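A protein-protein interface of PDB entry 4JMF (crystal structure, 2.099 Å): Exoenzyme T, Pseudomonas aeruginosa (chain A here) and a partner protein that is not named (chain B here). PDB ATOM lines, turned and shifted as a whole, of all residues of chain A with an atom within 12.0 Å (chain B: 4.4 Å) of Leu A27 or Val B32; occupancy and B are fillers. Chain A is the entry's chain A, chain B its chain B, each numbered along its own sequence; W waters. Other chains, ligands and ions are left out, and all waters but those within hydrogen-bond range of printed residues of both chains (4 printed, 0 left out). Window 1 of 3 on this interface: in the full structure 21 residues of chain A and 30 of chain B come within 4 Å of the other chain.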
ATOM      1  N   PRO A  21     -38.754  18.797  -4.187  1.00  0.00           N
ATOM      2  CA  PRO A  21     -37.380  18.310  -4.352  1.00  0.00           C
ATOM      3  C   PRO A  21     -37.353  17.006  -5.131  1.00  0.00           C
ATOM      4  O   PRO A  21     -38.295  16.215  -5.047  1.00  0.00           O
ATOM      5  CB  PRO A  21     -36.903  18.075  -2.908  1.00  0.00           C
ATOM      6  CG  PRO A  21     -38.132  18.140  -2.054  1.00  0.00           C
ATOM      7  CD  PRO A  21     -39.080  19.053  -2.773  1.00  0.00           C
ATOM      8  N   LYS A  22     -36.299  16.785  -5.903  1.00  0.00           N
ATOM      9  CA  LYS A  22     -36.176  15.515  -6.604  1.00  0.00           C
ATOM     10  C   LYS A  22     -34.742  14.999  -6.587  1.00  0.00           C
ATOM     11  O   LYS A  22     -33.794  15.766  -6.395  1.00  0.00           O
ATOM     12  CB  LYS A  22     -36.676  15.644  -8.042  1.00  0.00           C
ATOM     13  CG  LYS A  22     -35.966  16.737  -8.833  1.00  0.00           C
ATOM     14  CD  LYS A  22     -36.076  16.501 -10.346  1.00  0.00           C
ATOM     15  CE  LYS A  22     -35.517  17.703 -11.122  1.00  0.00           C
ATOM     16  NZ  LYS A  22     -34.010  17.858 -11.386  1.00  0.00           N
ATOM     17  N   GLY A  23     -34.593  13.695  -6.776  1.00  0.00           N
ATOM     18  CA  GLY A  23     -33.280  13.095  -6.904  1.00  0.00           C
ATOM     19  C   GLY A  23     -32.585  12.855  -5.582  1.00  0.00           C
ATOM     20  O   GLY A  23     -31.390  12.544  -5.546  1.00  0.00           O
ATOM     21  N   GLU A  24     -33.316  13.009  -4.484  1.00  0.00           N
ATOM     22  CA  GLU A  24     -32.728  12.726  -3.176  1.00  0.00           C
ATOM     23  C   GLU A  24     -32.224  11.276  -3.134  1.00  0.00           C
ATOM     24  O   GLU A  24     -32.956  10.345  -3.491  1.00  0.00           O
ATOM     25  CB  GLU A  24     -33.730  13.052  -2.066  1.00  0.00           C
ATOM     26  CG  GLU A  24     -34.395  14.422  -2.316  1.00  0.00           C
ATOM     27  CD  GLU A  24     -35.025  15.042  -1.082  1.00  0.00           C
ATOM     28  OE1 GLU A  24     -36.180  14.681  -0.763  1.00  0.00           O
ATOM     29  OE2 GLU A  24     -34.372  15.909  -0.448  1.00  0.00           O
ATOM     30  N   GLY A  25     -30.949  11.105  -2.769  1.00  0.00           N
ATOM     31  CA  GLY A  25     -30.316   9.795  -2.730  1.00  0.00           C
ATOM     32  C   GLY A  25     -30.078   9.150  -4.095  1.00  0.00           C
ATOM     33  O   GLY A  25     -29.583   8.018  -4.173  1.00  0.00           O
ATOM     34  N   LEU A  26     -30.413   9.858  -5.174  1.00  0.00           N
ATOM     35  CA  LEU A  26     -30.305   9.282  -6.525  1.00  0.00           C
ATOM     36  C   LEU A  26     -28.870   8.957  -6.957  1.00  0.00           C
ATOM     37  O   LEU A  26     -28.623   7.886  -7.524  1.00  0.00           O
ATOM     38  CB  LEU A  26     -30.948  10.210  -7.551  1.00  0.00           C
ATOM     39  CG  LEU A  26     -30.976   9.693  -8.984  1.00  0.00           C
ATOM     40  CD1 LEU A  26     -31.824   8.441  -9.072  1.00  0.00           C
ATOM     41  CD2 LEU A  26     -31.512  10.778  -9.903  1.00  0.00           C
ATOM     42  N   LEU A  27     -27.923   9.869  -6.711  1.00  0.00           N
ATOM     43  CA  LEU A  27     -26.529   9.583  -7.084  1.00  0.00           C
ATOM     44  C   LEU A  27     -25.985   8.358  -6.326  1.00  0.00           C
ATOM     45  O   LEU A  27     -25.299   7.512  -6.911  1.00  0.00           O
ATOM     46  CB  LEU A  27     -25.614  10.805  -6.907  1.00  0.00           C
ATOM     47  CG  LEU A  27     -25.843  12.010  -7.836  1.00  0.00           C
ATOM     48  CD1 LEU A  27     -24.794  13.081  -7.610  1.00  0.00           C
ATOM     49  CD2 LEU A  27     -25.848  11.594  -9.300  1.00  0.00           C
ATOM     50  N   SER A  28     -26.292   8.259  -5.034  1.00  0.00           N
ATOM     51  CA  SER A  28     -25.862   7.089  -4.246  1.00  0.00           C
ATOM     52  C   SER A  28     -26.467   5.791  -4.777  1.00  0.00           C
ATOM     53  O   SER A  28     -25.807   4.757  -4.807  1.00  0.00           O
ATOM     54  CB  SER A  28     -26.205   7.264  -2.766  1.00  0.00           C
ATOM     55  OG  SER A  28     -25.428   8.303  -2.194  1.00  0.00           O
ATOM     56  N   ARG A  29     -27.716   5.854  -5.220  1.00  0.00           N
ATOM     57  CA  ARG A  29     -28.393   4.668  -5.726  1.00  0.00           C
ATOM     58  C   ARG A  29     -27.868   4.194  -7.088  1.00  0.00           C
ATOM     59  O   ARG A  29     -27.658   2.998  -7.283  1.00  0.00           O
ATOM     60  CB  ARG A  29     -29.908   4.906  -5.765  1.00  0.00           C
ATOM     61  CG  ARG A  29     -30.724   3.706  -6.197  1.00  0.00           C
ATOM     62  CD  ARG A  29     -32.210   3.903  -5.910  1.00  0.00           C
ATOM     63  NE  ARG A  29     -32.679   5.258  -6.202  1.00  0.00           N
ATOM     64  CZ  ARG A  29     -33.021   6.152  -5.274  1.00  0.00           C
ATOM     65  NH1 ARG A  29     -32.946   5.840  -3.982  1.00  0.00           N
ATOM     66  NH2 ARG A  29     -33.435   7.363  -5.634  1.00  0.00           N
ATOM     67  N   LEU A  30     -27.647   5.120  -8.025  1.00  0.00           N
ATOM     68  CA  LEU A  30     -27.188   4.747  -9.369  1.00  0.00           C
ATOM     69  C   LEU A  30     -25.686   4.450  -9.427  1.00  0.00           C
ATOM     70  O   LEU A  30     -25.228   3.686 -10.275  1.00  0.00           O
ATOM     71  CB  LEU A  30     -27.527   5.844 -10.390  1.00  0.00           C
ATOM     72  CG  LEU A  30     -28.993   6.120 -10.719  1.00  0.00           C
ATOM     73  CD1 LEU A  30     -29.106   7.273 -11.694  1.00  0.00           C
ATOM     74  CD2 LEU A  30     -29.651   4.889 -11.307  1.00  0.00           C
ATOM     75  N   GLY A  31     -24.917   5.075  -8.545  1.00  0.00           N
ATOM     76  CA  GLY A  31     -23.469   4.947  -8.592  1.00  0.00           C
ATOM     77  C   GLY A  31     -22.875   5.778  -9.718  1.00  0.00           C
ATOM     78  O   GLY A  31     -23.587   6.188 -10.641  1.00  0.00           O
ATOM     79  N   ALA A  32     -21.575   6.030  -9.648  1.00  0.00           N
ATOM     80  CA  ALA A  32     -20.888   6.795 -10.683  1.00  0.00           C
ATOM     81  C   ALA A  32     -19.486   6.253 -10.919  1.00  0.00           C
ATOM     82  O   ALA A  32     -18.834   5.780  -9.993  1.00  0.00           O
ATOM     83  CB  ALA A  32     -20.811   8.251 -10.297  1.00  0.00           C
ATOM     84  N   ALA A  33     -19.025   6.336 -12.160  1.00  0.00           N
ATOM     85  CA  ALA A  33     -17.672   5.923 -12.506  1.00  0.00           C
ATOM     86  C   ALA A  33     -17.125   6.893 -13.541  1.00  0.00           C
ATOM     87  O   ALA A  33     -17.897   7.537 -14.260  1.00  0.00           O
ATOM     88  CB  ALA A  33     -17.683   4.511 -13.070  1.00  0.00           C
ATOM     89  N   LEU A  34     -15.804   6.996 -13.634  1.00  0.00           N
ATOM     90  CA  LEU A  34     -15.198   7.803 -14.676  1.00  0.00           C
ATOM     91  C   LEU A  34     -15.593   7.141 -15.983  1.00  0.00           C
ATOM     92  O   LEU A  34     -15.839   5.932 -16.015  1.00  0.00           O
ATOM     93  CB  LEU A  34     -13.673   7.829 -14.532  1.00  0.00           C
ATOM     94  CG  LEU A  34     -12.895   8.873 -15.346  1.00  0.00           C
ATOM     95  CD1 LEU A  34     -13.278  10.313 -14.970  1.00  0.00           C
ATOM     96  CD2 LEU A  34     -11.393   8.666 -15.169  1.00  0.00           C
ATOM     97  N   ALA A  35     -15.700   7.925 -17.052  1.00  0.00           N
ATOM     98  CA  ALA A  35     -16.023   7.357 -18.353  1.00  0.00           C
ATOM     99  C   ALA A  35     -14.946   7.723 -19.364  1.00  0.00           C
ATOM    100  O   ALA A  35     -14.296   8.768 -19.240  1.00  0.00           O
ATOM    101  CB  ALA A  35     -17.407   7.830 -18.831  1.00  0.00           C
ATOM    102  N   ARG A  36     -14.772   6.860 -20.364  1.00  0.00           N
ATOM    103  CA  ARG A  36     -13.828   7.092 -21.449  1.00  0.00           C
ATOM    104  C   ARG A  36     -14.577   7.017 -22.763  1.00  0.00           C
ATOM    105  O   ARG A  36     -14.501   6.008 -23.463  1.00  0.00           O
ATOM    106  CB  ARG A  36     -12.733   6.019 -21.465  1.00  0.00           C
ATOM    107  CG  ARG A  36     -11.797   5.986 -20.267  1.00  0.00           C
ATOM    108  CD  ARG A  36     -10.562   5.104 -20.553  1.00  0.00           C
ATOM    109  NE  ARG A  36      -9.714   5.661 -21.613  1.00  0.00           N
ATOM    110  CZ  ARG A  36      -8.692   6.493 -21.401  1.00  0.00           C
ATOM    111  NH1 ARG A  36      -8.375   6.864 -20.164  1.00  0.00           N
ATOM    112  NH2 ARG A  36      -7.981   6.957 -22.423  1.00  0.00           N
ATOM    113  N   PRO A  37     -15.308   8.080 -23.114  1.00  0.00           N
ATOM    114  CA  PRO A  37     -16.123   7.983 -24.333  1.00  0.00           C
ATOM    115  C   PRO A  37     -15.278   8.206 -25.583  1.00  0.00           C
ATOM    116  O   PRO A  37     -14.136   8.648 -25.432  1.00  0.00           O
ATOM    117  CB  PRO A  37     -17.154   9.110 -24.156  1.00  0.00           C
ATOM    118  CG  PRO A  37     -16.505  10.099 -23.232  1.00  0.00           C
ATOM    119  CD  PRO A  37     -15.478   9.364 -22.406  1.00  0.00           C
ATOM    120  N   LEU B  16     -18.435  11.874  -4.845  1.00  0.00           N
ATOM    121  CA  LEU B  16     -18.881  10.675  -5.556  1.00  0.00           C
ATOM    122  C   LEU B  16     -18.042   9.448  -5.212  1.00  0.00           C
ATOM    123  O   LEU B  16     -18.303   8.354  -5.730  1.00  0.00           O
ATOM    124  CB  LEU B  16     -18.799  10.907  -7.065  1.00  0.00           C
ATOM    125  CG  LEU B  16     -19.645  12.054  -7.598  1.00  0.00           C
ATOM    126  CD1 LEU B  16     -19.273  12.317  -9.059  1.00  0.00           C
ATOM    127  CD2 LEU B  16     -21.119  11.696  -7.458  1.00  0.00           C
ATOM    128  N   LEU B  30     -18.522  11.399 -16.969  1.00  0.00           N
ATOM    129  CA  LEU B  30     -18.878  10.465 -15.906  1.00  0.00           C
ATOM    130  C   LEU B  30     -20.048   9.609 -16.355  1.00  0.00           C
ATOM    131  O   LEU B  30     -20.980  10.115 -16.965  1.00  0.00           O
ATOM    132  CB  LEU B  30     -19.318  11.235 -14.667  1.00  0.00           C
ATOM    133  CG  LEU B  30     -18.251  12.058 -13.967  1.00  0.00           C
ATOM    134  CD1 LEU B  30     -18.896  12.878 -12.864  1.00  0.00           C
ATOM    135  CD2 LEU B  30     -17.204  11.103 -13.399  1.00  0.00           C
ATOM    136  N   GLN B  31     -20.002   8.313 -16.062  1.00  0.00           N
ATOM    137  CA  GLN B  31     -21.146   7.441 -16.287  1.00  0.00           C
ATOM    138  C   GLN B  31     -21.928   7.326 -14.983  1.00  0.00           C
ATOM    139  O   GLN B  31     -21.423   6.800 -13.993  1.00  0.00           O
ATOM    140  CB  GLN B  31     -20.681   6.056 -16.722  1.00  0.00           C
ATOM    141  CG  GLN B  31     -21.816   5.160 -17.203  1.00  0.00           C
ATOM    142  CD  GLN B  31     -22.301   5.574 -18.572  1.00  0.00           C
ATOM    143  OE1 GLN B  31     -21.497   5.798 -19.480  1.00  0.00           O
ATOM    144  NE2 GLN B  31     -23.618   5.709 -18.724  1.00  0.00           N
ATOM    145  N   VAL B  32     -23.146   7.845 -14.958  1.00  0.00           N
ATOM    146  CA  VAL B  32     -23.967   7.750 -13.759  1.00  0.00           C
ATOM    147  C   VAL B  32     -25.174   6.901 -14.107  1.00  0.00           C
ATOM    148  O   VAL B  32     -26.129   7.382 -14.725  1.00  0.00           O
ATOM    149  CB  VAL B  32     -24.407   9.140 -13.247  1.00  0.00           C
ATOM    150  CG1 VAL B  32     -25.284   9.001 -12.024  1.00  0.00           C
ATOM    151  CG2 VAL B  32     -23.189   9.990 -12.915  1.00  0.00           C
ATOM    152  N   GLY B  33     -25.121   5.625 -13.746  1.00  0.00           N
ATOM    153  CA  GLY B  33     -26.122   4.687 -14.222  1.00  0.00           C
ATOM    154  C   GLY B  33     -26.112   4.730 -15.737  1.00  0.00           C
ATOM    155  O   GLY B  33     -25.051   4.721 -16.360  1.00  0.00           O
ATOM    156  N   PRO B  34     -27.295   4.829 -16.342  1.00  0.00           N
ATOM    157  CA  PRO B  34     -27.349   4.841 -17.809  1.00  0.00           C
ATOM    158  C   PRO B  34     -27.000   6.202 -18.430  1.00  0.00           C
ATOM    159  O   PRO B  34     -26.944   6.334 -19.663  1.00  0.00           O
ATOM    160  CB  PRO B  34     -28.798   4.458 -18.103  1.00  0.00           C
ATOM    161  CG  PRO B  34     -29.567   4.886 -16.885  1.00  0.00           C
ATOM    162  CD  PRO B  34     -28.630   4.852 -15.715  1.00  0.00           C
ATOM    163  N   HIS B  35     -26.727   7.193 -17.589  1.00  0.00           N
ATOM    164  CA  HIS B  35     -26.464   8.548 -18.080  1.00  0.00           C
ATOM    165  C   HIS B  35     -24.981   8.916 -18.201  1.00  0.00           C
ATOM    166  O   HIS B  35     -24.246   8.948 -17.204  1.00  0.00           O
ATOM    167  CB  HIS B  35     -27.177   9.542 -17.172  1.00  0.00           C
ATOM    168  CG  HIS B  35     -28.613   9.200 -16.940  1.00  0.00           C
ATOM    169  ND1 HIS B  35     -29.566   9.276 -17.937  1.00  0.00           N
ATOM    170  CD2 HIS B  35     -29.258   8.762 -15.832  1.00  0.00           C
ATOM    171  CE1 HIS B  35     -30.736   8.905 -17.448  1.00  0.00           C
ATOM    172  NE2 HIS B  35     -30.576   8.588 -16.174  1.00  0.00           N
ATOM    173  N   HIS B 102     -22.096  18.323  -5.737  1.00  0.00           N
ATOM    174  CA  HIS B 102     -22.819  17.056  -5.706  1.00  0.00           C
ATOM    175  C   HIS B 102     -24.279  17.307  -6.091  1.00  0.00           C
ATOM    176  O   HIS B 102     -24.842  16.608  -6.932  1.00  0.00           O
ATOM    177  CB  HIS B 102     -22.707  16.436  -4.306  1.00  0.00           C
ATOM    178  CG  HIS B 102     -23.370  15.098  -4.168  1.00  0.00           C
ATOM    179  ND1 HIS B 102     -24.669  14.953  -3.727  1.00  0.00           N
ATOM    180  CD2 HIS B 102     -22.901  13.844  -4.378  1.00  0.00           C
ATOM    181  CE1 HIS B 102     -24.977  13.668  -3.690  1.00  0.00           C
ATOM    182  NE2 HIS B 102     -23.923  12.974  -4.081  1.00  0.00           N
ATOM    183  N   LEU B 105     -24.903  17.931  -9.931  1.00  0.00           N
ATOM    184  CA  LEU B 105     -24.921  16.728 -10.751  1.00  0.00           C
ATOM    185  C   LEU B 105     -26.202  15.934 -10.498  1.00  0.00           C
ATOM    186  O   LEU B 105     -26.808  15.397 -11.434  1.00  0.00           O
ATOM    187  CB  LEU B 105     -23.679  15.865 -10.482  1.00  0.00           C
ATOM    188  CG  LEU B 105     -23.571  14.545 -11.256  1.00  0.00           C
ATOM    189  CD1 LEU B 105     -23.518  14.793 -12.777  1.00  0.00           C
ATOM    190  CD2 LEU B 105     -22.335  13.753 -10.802  1.00  0.00           C
ATOM    191  N   GLU B 106     -26.623  15.878  -9.239  1.00  0.00           N
ATOM    192  CA  GLU B 106     -27.789  15.087  -8.876  1.00  0.00           C
ATOM    193  C   GLU B 106     -29.044  15.615  -9.544  1.00  0.00           C
ATOM    194  O   GLU B 106     -29.863  14.829 -10.030  1.00  0.00           O
ATOM    195  CB  GLU B 106     -27.977  15.076  -7.359  1.00  0.00           C
ATOM    196  CG  GLU B 106     -29.006  14.056  -6.873  1.00  0.00           C
ATOM    197  CD  GLU B 106     -28.681  13.560  -5.475  1.00  0.00           C
ATOM    198  OE1 GLU B 106     -28.881  14.326  -4.499  1.00  0.00           O
ATOM    199  OE2 GLU B 106     -28.215  12.401  -5.358  1.00  0.00           O
ATOM    200  N   VAL B 109     -28.934  14.610 -13.234  1.00  0.00           N
ATOM    201  CA  VAL B 109     -29.305  13.207 -13.384  1.00  0.00           C
ATOM    202  C   VAL B 109     -30.776  12.940 -13.049  1.00  0.00           C
ATOM    203  O   VAL B 109     -31.434  12.139 -13.719  1.00  0.00           O
ATOM    204  CB  VAL B 109     -28.359  12.291 -12.587  1.00  0.00           C
ATOM    205  CG1 VAL B 109     -28.825  10.853 -12.672  1.00  0.00           C
ATOM    206  CG2 VAL B 109     -26.956  12.402 -13.162  1.00  0.00           C
HETATM  207  O   HOH W   1     -22.488   3.807 -12.555  1.00  0.00           O
HETATM  208  O   HOH W   2     -27.182  10.467  -3.658  1.00  0.00           O
HETATM  209  O   HOH W   3     -29.424  13.448  -2.115  1.00  0.00           O
HETATM  210  O   HOH W   4     -23.658  10.031  -3.992  1.00  0.00           O
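The side-chain carboxylate (OE2) of Glu B106 is in hydrogen-bond range of the backbone NH (N) of Leu A26, 3.4 Å away.
The backbone NH (N) of Leu A27 lies within hydrogen-bond range of the side-chain carboxylate (OE2) of Glu B106 (2.9 Å).
The side-chain carboxylate (OE2) of Glu B106 lies close to the backbone carbonyl oxygen (O) of Gly A23 (3.2 Å).
O of Ala A33 is in hydrogen-bond range of N of Gln B31, at 2.9 Å.
The side-chain amide nitrogen of Gln B31 sits at hydrogen-bond distance from the backbone carbonyl oxygen of Gly B33, at 2.9 Å.
C of Gly A25 touches OE2 of Glu B106 (3.95 Å).
Leu A26 touches Val B109.
Val B32 touches Leu A27 (CG1 to CD2, 3.8 Å).
Leu A27 touches His B102 (CD1 to O, 3.6 Å).
Gly B33 touches Leu A30 (N to O, 3.98 Å).
Gly A31 touches Val B32.
Gln B31 touches Ala A32.
Ala A32 touches Val B32.
O of Ala A33 touches CA of Leu B30, 3.5 Å away.
Ala A35 touches Gln B31 (CB to N, 3.8 Å).
Of the printed residues of chain B, Gly A23 touches Glu B106.
Ser A28 touches none of the printed residues of chain B.
Of the printed residues of chain B, Gly A31 touches Val B32 (3.5 Å) and Gly B33 (3.5 Å).
Of the printed residues of chain B, Ala A32 touches Gln B31 (3.4 Å) and Val B32 (3.9 Å).
Of the printed residues of chain B, Ala A33 touches Leu B30 (3.5 Å) and Gln B31 (2.9 Å).
Arg A36 touches none of the printed residues of chain B.
Of the printed residues of chain A, Leu B16 touches Leu A27 (3.9 Å).
Leu B30 touches one residue of chain A.
Gln B31 touches just these residues of chain A: Ala A32 (3.4 Å), Ala A33 (2.9 Å) and Ala A35 (3.8 Å).
Of chain A, only Leu A27 (3.8 Å), Gly A31 (3.5 Å) and Ala A32 (3.9 Å) come within 4 Å of Val B32.
Gly B33 touches just these residues of chain A: Leu A30 and Gly A31.
No residue of chain A comes within 4 Å of Pro B34.
No residue of chain A comes within 4 Å of His B35.
Of chain A, only Leu A26 (3.9 Å) and Leu A30 (3.7 Å) come within 4 Å of Val B109.
The nearest printed residue of chain B that does not touch Leu A27 is Leu B105 (4.1 Å).
Of the 11 printed residues of chain B, 8 touch a printed residue of chain A.
Hydrophobic or aromatic side chains of chain A within 4 Å of the printed part of chain B: Leu A26, Leu A27, Leu A30, Ala A32 and Ala A35.
Among the printed residues, no Asp or Glu carboxylate lies within 4 Å of a Lys or Arg side-chain nitrogen of the other chain.
Water W3 bridges OE1 of Glu B106 (2.6 Å) and N of Gly A25 (2.9 Å).
Water W2 lies within hydrogen-bond range of N of Ser A28, OE2 of Glu B106, N of Leu A27 and O of Gly A25.
Water W4 bridges NE2 of His B102 and OG of Ser A28.
Water W1 lies within hydrogen-bond range of the backbone carbonyl oxygen (O) of Gly A31 (3.2 Å), the backbone NH (N) of Gly B33 (3.4 Å) and the backbone carbonyl oxygen (O) of Gln B31 (3.5 Å).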
